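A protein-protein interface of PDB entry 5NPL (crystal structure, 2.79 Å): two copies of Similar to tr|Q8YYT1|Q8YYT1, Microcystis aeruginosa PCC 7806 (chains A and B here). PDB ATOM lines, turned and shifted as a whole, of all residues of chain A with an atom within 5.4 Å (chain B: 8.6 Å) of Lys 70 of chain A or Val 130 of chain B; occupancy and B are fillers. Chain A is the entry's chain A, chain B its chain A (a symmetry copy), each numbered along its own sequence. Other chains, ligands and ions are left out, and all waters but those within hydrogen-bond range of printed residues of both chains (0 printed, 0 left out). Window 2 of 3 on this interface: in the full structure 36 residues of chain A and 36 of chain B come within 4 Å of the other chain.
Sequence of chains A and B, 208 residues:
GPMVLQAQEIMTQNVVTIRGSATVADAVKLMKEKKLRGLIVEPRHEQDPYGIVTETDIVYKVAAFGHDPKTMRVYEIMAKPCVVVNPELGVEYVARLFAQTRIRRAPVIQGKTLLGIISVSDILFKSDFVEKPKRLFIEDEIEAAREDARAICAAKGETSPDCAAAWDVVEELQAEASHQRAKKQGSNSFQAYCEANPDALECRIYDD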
ATOM      1  N   THR A  23      -2.490  -6.098  16.924  1.00  0.00           N
ATOM      2  CA  THR A  23      -1.667  -7.271  16.627  1.00  0.00           C
ATOM      3  C   THR A  23      -1.871  -7.694  15.186  1.00  0.00           C
ATOM      4  O   THR A  23      -2.814  -7.283  14.542  1.00  0.00           O
ATOM      5  CB  THR A  23      -1.984  -8.459  17.540  1.00  0.00           C
ATOM      6  OG1 THR A  23      -3.371  -8.824  17.405  1.00  0.00           O
ATOM      7  CG2 THR A  23      -1.642  -8.083  18.998  1.00  0.00           C
ATOM      8  N   ALA A  25      -2.498 -10.706  14.392  1.00  0.00           N
ATOM      9  CA  ALA A  25      -3.679 -11.562  14.512  1.00  0.00           C
ATOM     10  C   ALA A  25      -5.000 -10.797  14.325  1.00  0.00           C
ATOM     11  O   ALA A  25      -5.850 -11.228  13.529  1.00  0.00           O
ATOM     12  CB  ALA A  25      -3.659 -12.291  15.822  1.00  0.00           C
ATOM     13  N   VAL A  28      -5.266 -10.034  10.696  1.00  0.00           N
ATOM     14  CA  VAL A  28      -5.606 -11.214   9.903  1.00  0.00           C
ATOM     15  C   VAL A  28      -7.101 -11.544  10.052  1.00  0.00           C
ATOM     16  O   VAL A  28      -7.765 -11.924   9.071  1.00  0.00           O
ATOM     17  CB  VAL A  28      -4.720 -12.434  10.255  1.00  0.00           C
ATOM     18  CG1 VAL A  28      -5.223 -13.697   9.535  1.00  0.00           C
ATOM     19  CG2 VAL A  28      -3.261 -12.164   9.878  1.00  0.00           C
ATOM     20  N   ASP A  68       4.724 -15.527  15.710  1.00  0.00           N
ATOM     21  CA  ASP A  68       3.423 -15.598  16.338  1.00  0.00           C
ATOM     22  C   ASP A  68       2.654 -14.318  16.021  1.00  0.00           C
ATOM     23  O   ASP A  68       2.987 -13.268  16.562  1.00  0.00           O
ATOM     24  CB  ASP A  68       3.597 -15.734  17.853  1.00  0.00           C
ATOM     25  CG  ASP A  68       2.302 -16.114  18.578  1.00  0.00           C
ATOM     26  OD1 ASP A  68       1.205 -15.977  18.046  1.00  0.00           O
ATOM     27  OD2 ASP A  68       2.368 -16.540  19.735  1.00  0.00           O
ATOM     28  N   PRO A  69       1.603 -14.395  15.179  1.00  0.00           N
ATOM     29  CA  PRO A  69       0.875 -13.169  14.926  1.00  0.00           C
ATOM     30  C   PRO A  69       0.241 -12.517  16.161  1.00  0.00           C
ATOM     31  O   PRO A  69      -0.087 -11.350  16.092  1.00  0.00           O
ATOM     32  CB  PRO A  69      -0.217 -13.600  13.934  1.00  0.00           C
ATOM     33  CG  PRO A  69       0.264 -14.838  13.354  1.00  0.00           C
ATOM     34  CD  PRO A  69       0.980 -15.524  14.482  1.00  0.00           C
ATOM     35  N   LYS A  70       0.059 -13.262  17.247  1.00  0.00           N
ATOM     36  CA  LYS A  70      -0.520 -12.712  18.479  1.00  0.00           C
ATOM     37  C   LYS A  70       0.421 -11.805  19.278  1.00  0.00           C
ATOM     38  O   LYS A  70      -0.043 -11.072  20.135  1.00  0.00           O
ATOM     39  CB  LYS A  70      -1.057 -13.837  19.379  1.00  0.00           C
ATOM     40  CG  LYS A  70      -2.205 -14.599  18.720  1.00  0.00           C
ATOM     41  CD  LYS A  70      -2.762 -15.739  19.568  1.00  0.00           C
ATOM     42  CE  LYS A  70      -1.747 -16.875  19.768  1.00  0.00           C
ATOM     43  NZ  LYS A  70      -1.029 -17.431  18.562  1.00  0.00           N
ATOM     44  N   THR A  71       1.729 -11.872  19.001  1.00  0.00           N
ATOM     45  CA  THR A  71       2.724 -11.004  19.645  1.00  0.00           C
ATOM     46  C   THR A  71       3.315  -9.940  18.719  1.00  0.00           C
ATOM     47  O   THR A  71       3.782  -8.916  19.195  1.00  0.00           O
ATOM     48  CB  THR A  71       3.921 -11.787  20.253  1.00  0.00           C
ATOM     49  OG1 THR A  71       4.898 -12.041  19.239  1.00  0.00           O
ATOM     50  CG2 THR A  71       3.487 -13.104  20.916  1.00  0.00           C
ATOM     51  N   MET A  72       3.340 -10.156  17.418  1.00  0.00           N
ATOM     52  CA  MET A  72       3.756  -9.076  16.517  1.00  0.00           C
ATOM     53  C   MET A  72       2.624  -8.057  16.399  1.00  0.00           C
ATOM     54  O   MET A  72       1.472  -8.370  16.630  1.00  0.00           O
ATOM     55  CB  MET A  72       4.114  -9.604  15.136  1.00  0.00           C
ATOM     56  CG  MET A  72       5.341 -10.459  15.150  1.00  0.00           C
ATOM     57  SD  MET A  72       6.025 -10.677  13.525  1.00  0.00           S
ATOM     58  CE  MET A  72       6.884  -9.099  13.336  1.00  0.00           C
ATOM     59  N   VAL B  91       2.346 -25.349   4.697  1.00  0.00           N
ATOM     60  CA  VAL B  91       2.049 -23.987   4.236  1.00  0.00           C
ATOM     61  C   VAL B  91       3.108 -22.982   4.654  1.00  0.00           C
ATOM     62  O   VAL B  91       3.338 -22.008   3.971  1.00  0.00           O
ATOM     63  CB  VAL B  91       0.646 -23.466   4.633  1.00  0.00           C
ATOM     64  CG1 VAL B  91      -0.432 -24.371   4.033  1.00  0.00           C
ATOM     65  CG2 VAL B  91       0.519 -23.322   6.161  1.00  0.00           C
ATOM     66  N   ILE B 123      -2.942 -18.379   1.587  1.00  0.00           N
ATOM     67  CA  ILE B 123      -2.224 -18.437   2.875  1.00  0.00           C
ATOM     68  C   ILE B 123      -2.851 -17.517   3.947  1.00  0.00           C
ATOM     69  O   ILE B 123      -3.105 -17.954   5.067  1.00  0.00           O
ATOM     70  CB  ILE B 123      -0.721 -18.127   2.713  1.00  0.00           C
ATOM     71  CG1 ILE B 123      -0.066 -19.248   1.905  1.00  0.00           C
ATOM     72  CG2 ILE B 123      -0.048 -17.985   4.063  1.00  0.00           C
ATOM     73  CD1 ILE B 123       1.340 -18.968   1.419  1.00  0.00           C
ATOM     74  N   LEU B 124      -3.105 -16.258   3.605  1.00  0.00           N
ATOM     75  CA  LEU B 124      -3.691 -15.336   4.554  1.00  0.00           C
ATOM     76  C   LEU B 124      -5.042 -15.796   5.057  1.00  0.00           C
ATOM     77  O   LEU B 124      -5.329 -15.660   6.247  1.00  0.00           O
ATOM     78  CB  LEU B 124      -3.856 -13.947   3.922  1.00  0.00           C
ATOM     79  CG  LEU B 124      -4.487 -12.852   4.790  1.00  0.00           C
ATOM     80  CD1 LEU B 124      -3.573 -12.532   5.966  1.00  0.00           C
ATOM     81  CD2 LEU B 124      -4.752 -11.622   3.928  1.00  0.00           C
ATOM     82  N   LYS B 126      -6.599 -18.972   4.818  1.00  0.00           N
ATOM     83  CA  LYS B 126      -6.823 -20.372   5.178  1.00  0.00           C
ATOM     84  C   LYS B 126      -5.706 -21.074   5.968  1.00  0.00           C
ATOM     85  O   LYS B 126      -5.895 -22.181   6.473  1.00  0.00           O
ATOM     86  CB  LYS B 126      -7.148 -21.124   3.883  1.00  0.00           C
ATOM     87  CG  LYS B 126      -8.416 -20.614   3.248  1.00  0.00           C
ATOM     88  CD  LYS B 126      -8.764 -21.324   1.981  1.00  0.00           C
ATOM     89  CE  LYS B 126      -8.186 -20.566   0.790  1.00  0.00           C
ATOM     90  NZ  LYS B 126      -8.327 -21.285  -0.516  1.00  0.00           N
ATOM     91  N   SER B 127      -4.543 -20.449   6.093  1.00  0.00           N
ATOM     92  CA  SER B 127      -3.444 -21.030   6.872  1.00  0.00           C
ATOM     93  C   SER B 127      -3.819 -21.030   8.360  1.00  0.00           C
ATOM     94  O   SER B 127      -4.571 -20.182   8.832  1.00  0.00           O
ATOM     95  CB  SER B 127      -2.165 -20.214   6.680  1.00  0.00           C
ATOM     96  OG  SER B 127      -1.145 -20.642   7.559  1.00  0.00           O
ATOM     97  N   ASP B 128      -3.244 -21.994   9.078  1.00  0.00           N
ATOM     98  CA  ASP B 128      -3.425 -22.148  10.525  1.00  0.00           C
ATOM     99  C   ASP B 128      -2.345 -21.392  11.337  1.00  0.00           C
ATOM    100  O   ASP B 128      -2.146 -21.682  12.516  1.00  0.00           O
ATOM    101  CB  ASP B 128      -3.428 -23.655  10.879  1.00  0.00           C
ATOM    102  CG  ASP B 128      -2.082 -24.376  10.536  1.00  0.00           C
ATOM    103  OD1 ASP B 128      -1.141 -23.732   9.977  1.00  0.00           O
ATOM    104  OD2 ASP B 128      -1.967 -25.593  10.804  1.00  0.00           O
ATOM    105  N   PHE B 129      -1.644 -20.438  10.708  1.00  0.00           N
ATOM    106  CA  PHE B 129      -0.474 -19.797  11.307  1.00  0.00           C
ATOM    107  C   PHE B 129      -0.785 -18.888  12.517  1.00  0.00           C
ATOM    108  O   PHE B 129       0.114 -18.616  13.326  1.00  0.00           O
ATOM    109  CB  PHE B 129       0.375 -19.066  10.233  1.00  0.00           C
ATOM    110  CG  PHE B 129      -0.141 -17.710   9.810  1.00  0.00           C
ATOM    111  CD1 PHE B 129      -1.257 -17.595   9.013  1.00  0.00           C
ATOM    112  CD2 PHE B 129       0.503 -16.538  10.197  1.00  0.00           C
ATOM    113  CE1 PHE B 129      -1.745 -16.352   8.601  1.00  0.00           C
ATOM    114  CE2 PHE B 129       0.010 -15.297   9.826  1.00  0.00           C
ATOM    115  CZ  PHE B 129      -1.117 -15.197   9.017  1.00  0.00           C
ATOM    116  N   VAL B 130      -2.027 -18.430  12.662  1.00  0.00           N
ATOM    117  CA  VAL B 130      -2.379 -17.638  13.819  1.00  0.00           C
ATOM    118  C   VAL B 130      -2.448 -18.537  15.056  1.00  0.00           C
ATOM    119  O   VAL B 130      -1.865 -18.236  16.101  1.00  0.00           O
ATOM    120  CB  VAL B 130      -3.714 -16.885  13.627  1.00  0.00           C
ATOM    121  CG1 VAL B 130      -4.185 -16.236  14.929  1.00  0.00           C
ATOM    122  CG2 VAL B 130      -3.584 -15.837  12.523  1.00  0.00           C
ATOM    123  N   GLU B 131      -3.172 -19.638  14.919  1.00  0.00           N
ATOM    124  CA  GLU B 131      -3.445 -20.558  16.026  1.00  0.00           C
ATOM    125  C   GLU B 131      -2.338 -21.602  16.254  1.00  0.00           C
ATOM    126  O   GLU B 131      -2.137 -22.020  17.377  1.00  0.00           O
ATOM    127  CB  GLU B 131      -4.828 -21.223  15.872  1.00  0.00           C
ATOM    128  CG  GLU B 131      -5.003 -22.102  14.637  1.00  0.00           C
ATOM    129  CD  GLU B 131      -5.721 -21.425  13.465  1.00  0.00           C
ATOM    130  OE1 GLU B 131      -5.707 -20.182  13.367  1.00  0.00           O
ATOM    131  OE2 GLU B 131      -6.290 -22.161  12.627  1.00  0.00           O
ATOM    132  N   LYS B 132      -1.625 -21.999  15.197  1.00  0.00           N
ATOM    133  CA  LYS B 132      -0.459 -22.929  15.290  1.00  0.00           C
ATOM    134  C   LYS B 132       0.815 -22.317  14.665  1.00  0.00           C
ATOM    135  O   LYS B 132       1.310 -22.776  13.633  1.00  0.00           O
ATOM    136  CB  LYS B 132      -0.785 -24.271  14.617  1.00  0.00           C
ATOM    137  CG  LYS B 132      -2.086 -24.900  15.092  1.00  0.00           C
ATOM    138  N   PRO B 133       1.345 -21.260  15.271  1.00  0.00           N
ATOM    139  CA  PRO B 133       2.610 -20.729  14.807  1.00  0.00           C
ATOM    140  C   PRO B 133       3.763 -21.638  15.261  1.00  0.00           C
ATOM    141  O   PRO B 133       3.884 -21.951  16.429  1.00  0.00           O
ATOM    142  CB  PRO B 133       2.679 -19.359  15.489  1.00  0.00           C
ATOM    143  CG  PRO B 133       1.951 -19.557  16.774  1.00  0.00           C
ATOM    144  CD  PRO B 133       0.877 -20.584  16.489  1.00  0.00           C
ATOM    145  N   LYS B 134       4.591 -22.062  14.324  1.00  0.00           N
ATOM    146  CA  LYS B 134       5.810 -22.803  14.608  1.00  0.00           C
ATOM    147  C   LYS B 134       6.919 -22.159  13.855  1.00  0.00           C
ATOM    148  O   LYS B 134       6.793 -21.976  12.633  1.00  0.00           O
ATOM    149  CB  LYS B 134       5.693 -24.270  14.166  1.00  0.00           C
ATOM    150  CG  LYS B 134       6.810 -25.174  14.720  1.00  0.00           C
ATOM    151  CD  LYS B 134       6.856 -26.535  14.050  1.00  0.00           C
ATOM    152  CE  LYS B 134       7.527 -26.448  12.685  1.00  0.00           C
ATOM    153  NZ  LYS B 134       7.199 -27.635  11.844  1.00  0.00           N
ATOM    154  N   HIS B 179       4.286 -26.686  22.952  1.00  0.00           N
ATOM    155  CA  HIS B 179       3.284 -25.591  23.061  1.00  0.00           C
ATOM    156  C   HIS B 179       2.433 -25.350  21.790  1.00  0.00           C
ATOM    157  O   HIS B 179       1.210 -25.157  21.884  1.00  0.00           O
ATOM    158  CB  HIS B 179       3.958 -24.262  23.464  1.00  0.00           C
ATOM    159  CG  HIS B 179       3.018 -23.271  24.094  1.00  0.00           C
ATOM    160  ND1 HIS B 179       3.068 -22.942  25.437  1.00  0.00           N
ATOM    161  CD2 HIS B 179       1.995 -22.550  23.570  1.00  0.00           C
ATOM    162  CE1 HIS B 179       2.119 -22.060  25.710  1.00  0.00           C
ATOM    163  NE2 HIS B 179       1.456 -21.805  24.595  1.00  0.00           N
ATOM    164  N   GLN B 180       3.097 -25.357  20.625  1.00  0.00           N
ATOM    165  CA  GLN B 180       2.451 -25.266  19.283  1.00  0.00           C
ATOM    166  C   GLN B 180       2.057 -26.605  18.594  1.00  0.00           C
ATOM    167  O   GLN B 180       1.121 -26.616  17.790  1.00  0.00           O
ATOM    168  CB  GLN B 180       3.323 -24.435  18.329  1.00  0.00           C
ATOM    169  CG  GLN B 180       4.635 -25.089  17.883  1.00  0.00           C
ATOM    170  CD  GLN B 180       5.785 -24.105  17.869  1.00  0.00           C
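NZ of Lys 70 of chain A sits at hydrogen-bond distance from O of Val 130 of chain B.
The backbone NH (N) of Ala 25 of chain A is in hydrogen-bond range of the backbone carbonyl oxygen (O) of Pro 69 of chain A, at 3.0 Å.
The side-chain carboxylate (OD1) of Asp 68 of chain A lies within salt-bridge range of the side-chain amino group (NZ) of Lys 70 of chain A (2.7 Å).
The side-chain hydroxyl of Ser 127 of chain B sits at hydrogen-bond distance from the backbone NH of Phe 129 of chain B.
Among the printed residues, merely in contact across the chains: Val 28 of chain A with Leu 124 of chain B (3.8 Å), Val 28 of chain A with Phe 129 of chain B (3.8 Å), Asp 68 of chain A with Pro 133 of chain B (3.9 Å), Pro 69 of chain A with Phe 129 of chain B (3.4 Å) and Pro 69 of chain A with Val 130 of chain B (3.9 Å).
Printed residues of chain B within 4 Å of Val 28 of chain A: Leu 124 (3.8 Å) and Phe 129 (3.8 Å).
Of the printed residues of chain B, Asp 68 of chain A touches Pro 133.
Lys 70 of chain A touches just one residue of chain B: Val 130 (2.7 Å).
No residue of chain B comes within 4 Å of Thr 71 of chain A.
Of the printed residues of chain A, Leu 124 of chain B touches Val 28 (3.8 Å).
Of the printed residues of chain A, Phe 129 of chain B touches Val 28 and Pro 69.
Of chain A, only Pro 69 (3.9 Å) and Lys 70 (2.7 Å) come within 4 Å of Val 130 of chain B.
Of the printed residues of chain A, Pro 133 of chain B touches Asp 68 (3.9 Å).
The nearest residue of chain B that does not touch Lys 70 of chain A is Pro 133 of chain B (4.1 Å).
Hydrophobic or aromatic side chains of chain A that line the printed part of chain B: Val 28 and Pro 69.
Of the 14 printed residues of chain B, 4 touch a printed residue of chain A.
Among the printed residues, 6 pairs touch across the chains.
Among the printed residues, no Asp or Glu carboxylate lies within 4 Å of a Lys or Arg side-chain nitrogen of the other chain.
No position is printed for both chains.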
